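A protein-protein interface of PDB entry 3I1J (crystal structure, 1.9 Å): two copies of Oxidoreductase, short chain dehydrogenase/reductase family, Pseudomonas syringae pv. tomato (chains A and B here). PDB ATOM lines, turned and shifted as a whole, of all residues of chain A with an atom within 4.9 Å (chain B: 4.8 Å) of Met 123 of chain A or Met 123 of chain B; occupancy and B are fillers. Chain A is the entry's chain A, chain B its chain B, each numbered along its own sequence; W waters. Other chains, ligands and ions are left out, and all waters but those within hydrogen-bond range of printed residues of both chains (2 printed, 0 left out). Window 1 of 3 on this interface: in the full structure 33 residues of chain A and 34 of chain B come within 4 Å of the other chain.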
ATOM      1  N   PHE A 119     -29.485   8.677 -15.234  1.00  0.00           N
ATOM      2  CA  PHE A 119     -28.472   9.665 -14.836  1.00  0.00           C
ATOM      3  C   PHE A 119     -28.683  10.109 -13.366  1.00  0.00           C
ATOM      4  O   PHE A 119     -27.749  10.094 -12.564  1.00  0.00           O
ATOM      5  CB  PHE A 119     -28.451  10.886 -15.821  1.00  0.00           C
ATOM      6  CG  PHE A 119     -27.386  11.928 -15.502  1.00  0.00           C
ATOM      7  CD1 PHE A 119     -26.177  11.929 -16.168  1.00  0.00           C
ATOM      8  CD2 PHE A 119     -27.622  12.937 -14.543  1.00  0.00           C
ATOM      9  CE1 PHE A 119     -25.191  12.882 -15.866  1.00  0.00           C
ATOM     10  CE2 PHE A 119     -26.658  13.876 -14.235  1.00  0.00           C
ATOM     11  CZ  PHE A 119     -25.443  13.867 -14.919  1.00  0.00           C
ATOM     12  N   MET A 120     -29.893  10.519 -13.000  1.00  0.00           N
ATOM     13  CA  MET A 120     -30.092  11.066 -11.663  1.00  0.00           C
ATOM     14  C   MET A 120     -29.910  10.001 -10.573  1.00  0.00           C
ATOM     15  O   MET A 120     -29.367  10.280  -9.513  1.00  0.00           O
ATOM     16  CB  MET A 120     -31.470  11.754 -11.557  1.00  0.00           C
ATOM     17  CG  MET A 120     -31.604  12.893 -12.552  1.00  0.00           C
ATOM     18  SD  MET A 120     -33.243  13.902 -12.214  1.00  0.00           S
ATOM     19  CE  MET A 120     -34.399  12.849 -13.271  1.00  0.00           C
ATOM     20  N   GLN A 121     -30.297   8.760 -10.863  1.00  0.00           N
ATOM     21  CA  GLN A 121     -30.172   7.716  -9.865  1.00  0.00           C
ATOM     22  C   GLN A 121     -28.708   7.374  -9.609  1.00  0.00           C
ATOM     23  O   GLN A 121     -28.295   7.237  -8.469  1.00  0.00           O
ATOM     24  CB  GLN A 121     -30.939   6.461 -10.273  1.00  0.00           C
ATOM     25  CG  GLN A 121     -30.797   5.384  -9.217  1.00  0.00           C
ATOM     26  CD  GLN A 121     -31.968   4.433  -9.171  1.00  0.00           C
ATOM     27  OE1 GLN A 121     -32.117   3.580 -10.016  1.00  0.00           O
ATOM     28  NE2 GLN A 121     -32.788   4.573  -8.153  1.00  0.00           N
ATOM     29  N   VAL A 122     -27.914   7.280 -10.666  1.00  0.00           N
ATOM     30  CA  VAL A 122     -26.465   7.091 -10.512  1.00  0.00           C
ATOM     31  C   VAL A 122     -25.899   8.235  -9.651  1.00  0.00           C
ATOM     32  O   VAL A 122     -25.134   7.983  -8.704  1.00  0.00           O
ATOM     33  CB  VAL A 122     -25.708   6.983 -11.892  1.00  0.00           C
ATOM     34  CG1 VAL A 122     -24.126   6.922 -11.692  1.00  0.00           C
ATOM     35  CG2 VAL A 122     -26.215   5.775 -12.742  1.00  0.00           C
ATOM     36  N   MET A 123     -26.272   9.484  -9.957  1.00  0.00           N
ATOM     37  CA  MET A 123     -25.756  10.632  -9.185  1.00  0.00           C
ATOM     38  C   MET A 123     -26.226  10.558  -7.735  1.00  0.00           C
ATOM     39  O   MET A 123     -25.470  10.907  -6.788  1.00  0.00           O
ATOM     40  CB  MET A 123     -26.204  11.983  -9.786  1.00  0.00           C
ATOM     41  CG  MET A 123     -25.619  12.260 -11.187  1.00  0.00           C
ATOM     42  SD  MET A 123     -23.648  12.330 -11.232  1.00  0.00           S
ATOM     43  CE  MET A 123     -23.363  13.816 -10.040  1.00  0.00           C
ATOM     44  N   HIS A 124     -27.467  10.098  -7.563  1.00  0.00           N
ATOM     45  CA  HIS A 124     -27.985  10.007  -6.217  1.00  0.00           C
ATOM     46  C   HIS A 124     -27.183   8.976  -5.414  1.00  0.00           C
ATOM     47  O   HIS A 124     -26.679   9.278  -4.358  1.00  0.00           O
ATOM     48  CB  HIS A 124     -29.471   9.632  -6.170  1.00  0.00           C
ATOM     49  CG  HIS A 124     -29.985   9.662  -4.771  1.00  0.00           C
ATOM     50  ND1 HIS A 124     -30.305  10.843  -4.140  1.00  0.00           N
ATOM     51  CD2 HIS A 124     -30.067   8.691  -3.824  1.00  0.00           C
ATOM     52  CE1 HIS A 124     -30.665  10.586  -2.890  1.00  0.00           C
ATOM     53  NE2 HIS A 124     -30.527   9.288  -2.672  1.00  0.00           N
ATOM     54  N   VAL A 125     -27.043   7.772  -5.954  1.00  0.00           N
ATOM     55  CA  VAL A 125     -26.393   6.671  -5.235  1.00  0.00           C
ATOM     56  C   VAL A 125     -24.879   6.939  -5.013  1.00  0.00           C
ATOM     57  O   VAL A 125     -24.330   6.675  -3.933  1.00  0.00           O
ATOM     58  CB  VAL A 125     -26.658   5.312  -6.001  1.00  0.00           C
ATOM     59  CG1 VAL A 125     -25.859   4.126  -5.423  1.00  0.00           C
ATOM     60  CG2 VAL A 125     -28.153   4.953  -5.943  1.00  0.00           C
ATOM     61  N   ASN A 126     -24.196   7.406  -6.052  1.00  0.00           N
ATOM     62  CA  ASN A 126     -22.750   7.558  -5.996  1.00  0.00           C
ATOM     63  C   ASN A 126     -22.294   8.821  -5.279  1.00  0.00           C
ATOM     64  O   ASN A 126     -21.178   8.853  -4.723  1.00  0.00           O
ATOM     65  CB  ASN A 126     -22.132   7.488  -7.403  1.00  0.00           C
ATOM     66  CG  ASN A 126     -22.293   6.142  -8.062  1.00  0.00           C
ATOM     67  OD1 ASN A 126     -22.941   5.242  -7.528  1.00  0.00           O
ATOM     68  ND2 ASN A 126     -21.723   6.002  -9.274  1.00  0.00           N
ATOM     69  N   VAL A 127     -23.128   9.870  -5.290  1.00  0.00           N
ATOM     70  CA  VAL A 127     -22.715  11.134  -4.730  1.00  0.00           C
ATOM     71  C   VAL A 127     -23.610  11.557  -3.547  1.00  0.00           C
ATOM     72  O   VAL A 127     -23.081  11.815  -2.462  1.00  0.00           O
ATOM     73  CB  VAL A 127     -22.687  12.257  -5.814  1.00  0.00           C
ATOM     74  CG1 VAL A 127     -22.128  13.563  -5.203  1.00  0.00           C
ATOM     75  CG2 VAL A 127     -21.894  11.823  -7.052  1.00  0.00           C
ATOM     76  N   ASN A 128     -24.938  11.652  -3.753  1.00  0.00           N
ATOM     77  CA  ASN A 128     -25.823  12.176  -2.669  1.00  0.00           C
ATOM     78  C   ASN A 128     -25.711  11.276  -1.432  1.00  0.00           C
ATOM     79  O   ASN A 128     -25.524  11.747  -0.309  1.00  0.00           O
ATOM     80  CB  ASN A 128     -27.297  12.325  -3.108  1.00  0.00           C
ATOM     81  CG  ASN A 128     -27.500  13.422  -4.151  1.00  0.00           C
ATOM     82  OD1 ASN A 128     -26.593  14.215  -4.438  1.00  0.00           O
ATOM     83  ND2 ASN A 128     -28.671  13.452  -4.735  1.00  0.00           N
ATOM     84  N   ALA A 166     -23.418   8.608 -16.409  1.00  0.00           N
ATOM     85  CA  ALA A 166     -23.336   9.364 -15.175  1.00  0.00           C
ATOM     86  C   ALA A 166     -22.184   8.880 -14.311  1.00  0.00           C
ATOM     87  O   ALA A 166     -21.863   9.515 -13.324  1.00  0.00           O
ATOM     88  CB  ALA A 166     -24.636   9.277 -14.404  1.00  0.00           C
ATOM     89  N   VAL A 169     -19.064  11.287 -14.468  1.00  0.00           N
ATOM     90  CA  VAL A 169     -19.569  12.501 -13.823  1.00  0.00           C
ATOM     91  C   VAL A 169     -19.602  12.328 -12.308  1.00  0.00           C
ATOM     92  O   VAL A 169     -19.158  13.205 -11.586  1.00  0.00           O
ATOM     93  CB  VAL A 169     -20.985  12.902 -14.359  1.00  0.00           C
ATOM     94  CG1 VAL A 169     -21.463  14.189 -13.712  1.00  0.00           C
ATOM     95  CG2 VAL A 169     -20.939  13.095 -15.876  1.00  0.00           C
ATOM     96  N   SER A 170     -20.114  11.189 -11.836  1.00  0.00           N
ATOM     97  CA  SER A 170     -20.263  10.953 -10.381  1.00  0.00           C
ATOM     98  C   SER A 170     -18.904  10.843  -9.722  1.00  0.00           C
ATOM     99  O   SER A 170     -18.739  11.203  -8.548  1.00  0.00           O
ATOM    100  CB  SER A 170     -21.085   9.677 -10.124  1.00  0.00           C
ATOM    101  OG  SER A 170     -20.307   8.477 -10.274  1.00  0.00           O
ATOM    102  N   ALA A 173     -17.460  14.248  -9.348  1.00  0.00           N
ATOM    103  CA  ALA A 173     -18.075  14.820  -8.145  1.00  0.00           C
ATOM    104  C   ALA A 173     -17.388  14.256  -6.892  1.00  0.00           C
ATOM    105  O   ALA A 173     -17.038  15.011  -5.964  1.00  0.00           O
ATOM    106  CB  ALA A 173     -19.566  14.538  -8.134  1.00  0.00           C
ATOM    107  N   PHE B 119     -27.567  20.170  -0.226  1.00  0.00           N
ATOM    108  CA  PHE B 119     -26.559  19.483  -1.078  1.00  0.00           C
ATOM    109  C   PHE B 119     -27.275  18.899  -2.296  1.00  0.00           C
ATOM    110  O   PHE B 119     -26.856  19.139  -3.432  1.00  0.00           O
ATOM    111  CB  PHE B 119     -25.801  18.402  -0.290  1.00  0.00           C
ATOM    112  CG  PHE B 119     -24.771  17.667  -1.106  1.00  0.00           C
ATOM    113  CD1 PHE B 119     -23.428  18.039  -1.049  1.00  0.00           C
ATOM    114  CD2 PHE B 119     -25.146  16.611  -1.946  1.00  0.00           C
ATOM    115  CE1 PHE B 119     -22.456  17.369  -1.833  1.00  0.00           C
ATOM    116  CE2 PHE B 119     -24.175  15.937  -2.730  1.00  0.00           C
ATOM    117  CZ  PHE B 119     -22.844  16.329  -2.666  1.00  0.00           C
ATOM    118  N   MET B 120     -28.390  18.200  -2.066  1.00  0.00           N
ATOM    119  CA  MET B 120     -29.153  17.597  -3.154  1.00  0.00           C
ATOM    120  C   MET B 120     -29.702  18.621  -4.158  1.00  0.00           C
ATOM    121  O   MET B 120     -29.640  18.399  -5.372  1.00  0.00           O
ATOM    122  CB  MET B 120     -30.239  16.681  -2.587  1.00  0.00           C
ATOM    123  CG  MET B 120     -29.609  15.489  -1.885  1.00  0.00           C
ATOM    124  SD  MET B 120     -30.925  14.161  -1.406  1.00  0.00           S
ATOM    125  CE  MET B 120     -31.550  14.801   0.265  1.00  0.00           C
ATOM    126  N   GLN B 121     -30.177  19.756  -3.660  1.00  0.00           N
ATOM    127  CA  GLN B 121     -30.782  20.746  -4.513  1.00  0.00           C
ATOM    128  C   GLN B 121     -29.722  21.407  -5.401  1.00  0.00           C
ATOM    129  O   GLN B 121     -29.964  21.568  -6.587  1.00  0.00           O
ATOM    130  CB  GLN B 121     -31.514  21.782  -3.672  1.00  0.00           C
ATOM    131  CG  GLN B 121     -32.171  22.884  -4.497  1.00  0.00           C
ATOM    132  CD  GLN B 121     -32.755  23.941  -3.591  1.00  0.00           C
ATOM    133  OE1 GLN B 121     -32.026  24.750  -2.974  1.00  0.00           O
ATOM    134  NE2 GLN B 121     -34.068  23.947  -3.497  1.00  0.00           N
ATOM    135  N   VAL B 122     -28.564  21.750  -4.830  1.00  0.00           N
ATOM    136  CA  VAL B 122     -27.437  22.330  -5.596  1.00  0.00           C
ATOM    137  C   VAL B 122     -27.016  21.347  -6.686  1.00  0.00           C
ATOM    138  O   VAL B 122     -26.810  21.740  -7.857  1.00  0.00           O
ATOM    139  CB  VAL B 122     -26.231  22.722  -4.677  1.00  0.00           C
ATOM    140  CG1 VAL B 122     -25.013  23.239  -5.488  1.00  0.00           C
ATOM    141  CG2 VAL B 122     -26.647  23.812  -3.681  1.00  0.00           C
ATOM    142  N   MET B 123     -26.911  20.060  -6.322  1.00  0.00           N
ATOM    143  CA  MET B 123     -26.507  19.053  -7.319  1.00  0.00           C
ATOM    144  C   MET B 123     -27.567  18.961  -8.397  1.00  0.00           C
ATOM    145  O   MET B 123     -27.252  18.791  -9.573  1.00  0.00           O
ATOM    146  CB  MET B 123     -26.293  17.681  -6.697  1.00  0.00           C
ATOM    147  CG  MET B 123     -25.066  17.602  -5.750  1.00  0.00           C
ATOM    148  SD  MET B 123     -23.348  18.086  -6.572  1.00  0.00           S
ATOM    149  CE  MET B 123     -23.358  16.636  -7.842  1.00  0.00           C
ATOM    150  N   HIS B 124     -28.826  19.028  -8.002  1.00  0.00           N
ATOM    151  CA  HIS B 124     -29.875  18.912  -9.008  1.00  0.00           C
ATOM    152  C   HIS B 124     -29.864  20.102  -9.968  1.00  0.00           C
ATOM    153  O   HIS B 124     -29.924  19.943 -11.195  1.00  0.00           O
ATOM    154  CB  HIS B 124     -31.252  18.784  -8.376  1.00  0.00           C
ATOM    155  CG  HIS B 124     -32.293  18.392  -9.375  1.00  0.00           C
ATOM    156  ND1 HIS B 124     -33.045  19.318 -10.078  1.00  0.00           N
ATOM    157  CD2 HIS B 124     -32.592  17.186  -9.896  1.00  0.00           C
ATOM    158  CE1 HIS B 124     -33.820  18.679 -10.939  1.00  0.00           C
ATOM    159  NE2 HIS B 124     -33.572  17.386 -10.840  1.00  0.00           N
ATOM    160  N   VAL B 125     -29.808  21.300  -9.415  1.00  0.00           N
ATOM    161  CA  VAL B 125     -29.870  22.512 -10.271  1.00  0.00           C
ATOM    162  C   VAL B 125     -28.618  22.601 -11.145  1.00  0.00           C
ATOM    163  O   VAL B 125     -28.698  22.906 -12.353  1.00  0.00           O
ATOM    164  CB  VAL B 125     -30.076  23.819  -9.427  1.00  0.00           C
ATOM    165  CG1 VAL B 125     -29.839  25.108 -10.275  1.00  0.00           C
ATOM    166  CG2 VAL B 125     -31.463  23.818  -8.825  1.00  0.00           C
ATOM    167  N   ASN B 126     -27.463  22.301 -10.561  1.00  0.00           N
ATOM    168  CA  ASN B 126     -26.203  22.582 -11.273  1.00  0.00           C
ATOM    169  C   ASN B 126     -25.789  21.459 -12.210  1.00  0.00           C
ATOM    170  O   ASN B 126     -25.180  21.712 -13.235  1.00  0.00           O
ATOM    171  CB  ASN B 126     -25.076  22.932 -10.299  1.00  0.00           C
ATOM    172  CG  ASN B 126     -25.353  24.224  -9.549  1.00  0.00           C
ATOM    173  OD1 ASN B 126     -26.458  24.790  -9.644  1.00  0.00           O
ATOM    174  ND2 ASN B 126     -24.368  24.690  -8.793  1.00  0.00           N
ATOM    175  N   VAL B 127     -26.160  20.237 -11.861  1.00  0.00           N
ATOM    176  CA  VAL B 127     -25.700  19.046 -12.611  1.00  0.00           C
ATOM    177  C   VAL B 127     -26.830  18.340 -13.327  1.00  0.00           C
ATOM    178  O   VAL B 127     -26.774  18.174 -14.554  1.00  0.00           O
ATOM    179  CB  VAL B 127     -24.860  18.087 -11.728  1.00  0.00           C
ATOM    180  CG1 VAL B 127     -24.160  17.037 -12.597  1.00  0.00           C
ATOM    181  CG2 VAL B 127     -23.773  18.902 -10.950  1.00  0.00           C
ATOM    182  N   ASN B 128     -27.842  17.914 -12.575  1.00  0.00           N
ATOM    183  CA  ASN B 128     -28.964  17.188 -13.199  1.00  0.00           C
ATOM    184  C   ASN B 128     -29.702  18.001 -14.278  1.00  0.00           C
ATOM    185  O   ASN B 128     -29.991  17.491 -15.367  1.00  0.00           O
ATOM    186  CB  ASN B 128     -29.973  16.755 -12.167  1.00  0.00           C
ATOM    187  CG  ASN B 128     -29.463  15.655 -11.253  1.00  0.00           C
ATOM    188  OD1 ASN B 128     -28.346  15.127 -11.424  1.00  0.00           O
ATOM    189  ND2 ASN B 128     -30.273  15.321 -10.251  1.00  0.00           N
ATOM    190  N   ALA B 166     -21.899  22.304  -1.661  1.00  0.00           N
ATOM    191  CA  ALA B 166     -22.139  21.524  -2.863  1.00  0.00           C
ATOM    192  C   ALA B 166     -21.693  22.256  -4.128  1.00  0.00           C
ATOM    193  O   ALA B 166     -21.615  21.634  -5.199  1.00  0.00           O
ATOM    194  CB  ALA B 166     -23.600  21.098  -2.962  1.00  0.00           C
ATOM    195  N   VAL B 169     -18.321  20.897  -5.449  1.00  0.00           N
ATOM    196  CA  VAL B 169     -18.617  19.518  -5.890  1.00  0.00           C
ATOM    197  C   VAL B 169     -19.415  19.488  -7.205  1.00  0.00           C
ATOM    198  O   VAL B 169     -19.093  18.684  -8.099  1.00  0.00           O
ATOM    199  CB  VAL B 169     -19.366  18.700  -4.784  1.00  0.00           C
ATOM    200  CG1 VAL B 169     -19.696  17.229  -5.263  1.00  0.00           C
ATOM    201  CG2 VAL B 169     -18.596  18.694  -3.474  1.00  0.00           C
ATOM    202  N   SER B 170     -20.439  20.347  -7.329  1.00  0.00           N
ATOM    203  CA  SER B 170     -21.243  20.414  -8.557  1.00  0.00           C
ATOM    204  C   SER B 170     -20.434  20.898  -9.756  1.00  0.00           C
ATOM    205  O   SER B 170     -20.730  20.532 -10.893  1.00  0.00           O
ATOM    206  CB  SER B 170     -22.491  21.304  -8.375  1.00  0.00           C
ATOM    207  OG  SER B 170     -22.158  22.703  -8.554  1.00  0.00           O
ATOM    208  N   ALA B 173     -18.322  18.000 -11.039  1.00  0.00           N
ATOM    209  CA  ALA B 173     -19.240  17.168 -11.811  1.00  0.00           C
ATOM    210  C   ALA B 173     -19.460  17.730 -13.216  1.00  0.00           C
ATOM    211  O   ALA B 173     -19.465  16.991 -14.196  1.00  0.00           O
ATOM    212  CB  ALA B 173     -20.549  17.052 -11.065  1.00  0.00           C
HETATM  213  O   HOH W   1     -29.526  12.874  -8.407  1.00  0.00           O
HETATM  214  O   HOH W   2     -29.575  15.734  -6.343  1.00  0.00           O
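The side-chain sulfur (SD) of Met 120 of chain A lies within hydrogen-bond range of a ring nitrogen (NE2) of His 124 of chain B (3.8 Å).
N of Asn 128 of chain A is in hydrogen-bond range of O of Met 123 of chain A (3.2 Å). The side-chain sulfur of Met 123 of chain A sits close to the backbone NH of Ser 170 of chain A, at 3.8 Å. The side-chain amide nitrogen of Asn 128 of chain A lies within hydrogen-bond range of a ring nitrogen (ND1) of His 124 of chain A, 3.1 Å away. O of Met 123 of chain B is in hydrogen-bond range of N of Asn 128 of chain B. SD of Met 123 of chain B sits close to N of Ser 170 of chain B (3.8 Å).
Phe 119 of chain A touches Asn 128 of chain B (CE2 to OD1, 3.5 Å). Met 120 of chain A touches Asn 128 of chain B. Asn 128 of chain B touches Met 123 of chain A. Phe 119 of chain B touches Val 127 of chain A. OD1 of Asn 128 of chain A touches CE2 of Phe 119 of chain B (3.4 Å). Asn 128 of chain A touches Met 120 of chain B (ND2 to CG, 3.6 Å). OD1 of Asn 128 of chain A touches CG of Met 123 of chain B, at 3.9 Å. CG1 of Val 169 of chain A touches O of Ala 173 of chain B (3.5 Å). Ala 173 of chain A touches Val 169 of chain B (O to CG1, 3.5 Å). Ala 173 of chain A touches Ala 173 of chain B (CB to CB, 3.98 Å).
Met 123 of chain A touches just these residues of chain B: Met 123 and Asn 128. Of the printed residues of chain B, Phe 119 of chain A touches Asn 128. Of the printed residues of chain B, Met 120 of chain A touches His 124 and Asn 128. Ala 166 of chain B touches none of the printed residues of chain A. The nearest residue of chain A that does not touch Met 123 of chain B is Val 127 of chain A (4.2 Å).
Along chain A the printed residues that touch a printed residue of chain B span positions 119 to 173. Of the 14 printed residues of chain B, 7 touch a printed residue of chain A. Hydrophobic or aromatic side chains of chain B that line the printed part of chain A: Phe 119, Met 120, Met 123, His 124, Val 169 and Ala 173. Among the printed residues, 13 pairs touch across the chains. Among the printed residues, no Asp or Glu carboxylate lies within 4 Å of a Lys or Arg side-chain nitrogen of the other chain.
Phe 119 of chain A touches Asn 128 of chain B, and with the chains exchanged Asn 128 of chain A touches Phe 119 of chain B. Met 120 of chain A touches His 124 of chain B, and with the chains exchanged His 124 of chain A touches Met 120 of chain B. Met 123 of chain B touches its own counterpart, Met 123 of chain A. Met 123 of chain A touches Asn 128 of chain B, and with the chains exchanged Asn 128 of chain A touches Met 123 of chain B. 14 positions are printed for both chains. Of the 13 pairs that touch across the chains among the printed residues, 12 have their exchanged pair printed and touching as well.
Water W1 lies within hydrogen-bond range of the backbone carbonyl oxygen (O) of Met 120 of chain A and the side-chain amide nitrogen (ND2) of Asn 128 of chain B. Water W2 lies within hydrogen-bond range of O of Met 120 of chain B (2.8 Å) and ND2 of Asn 128 of chain A (2.9 Å).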
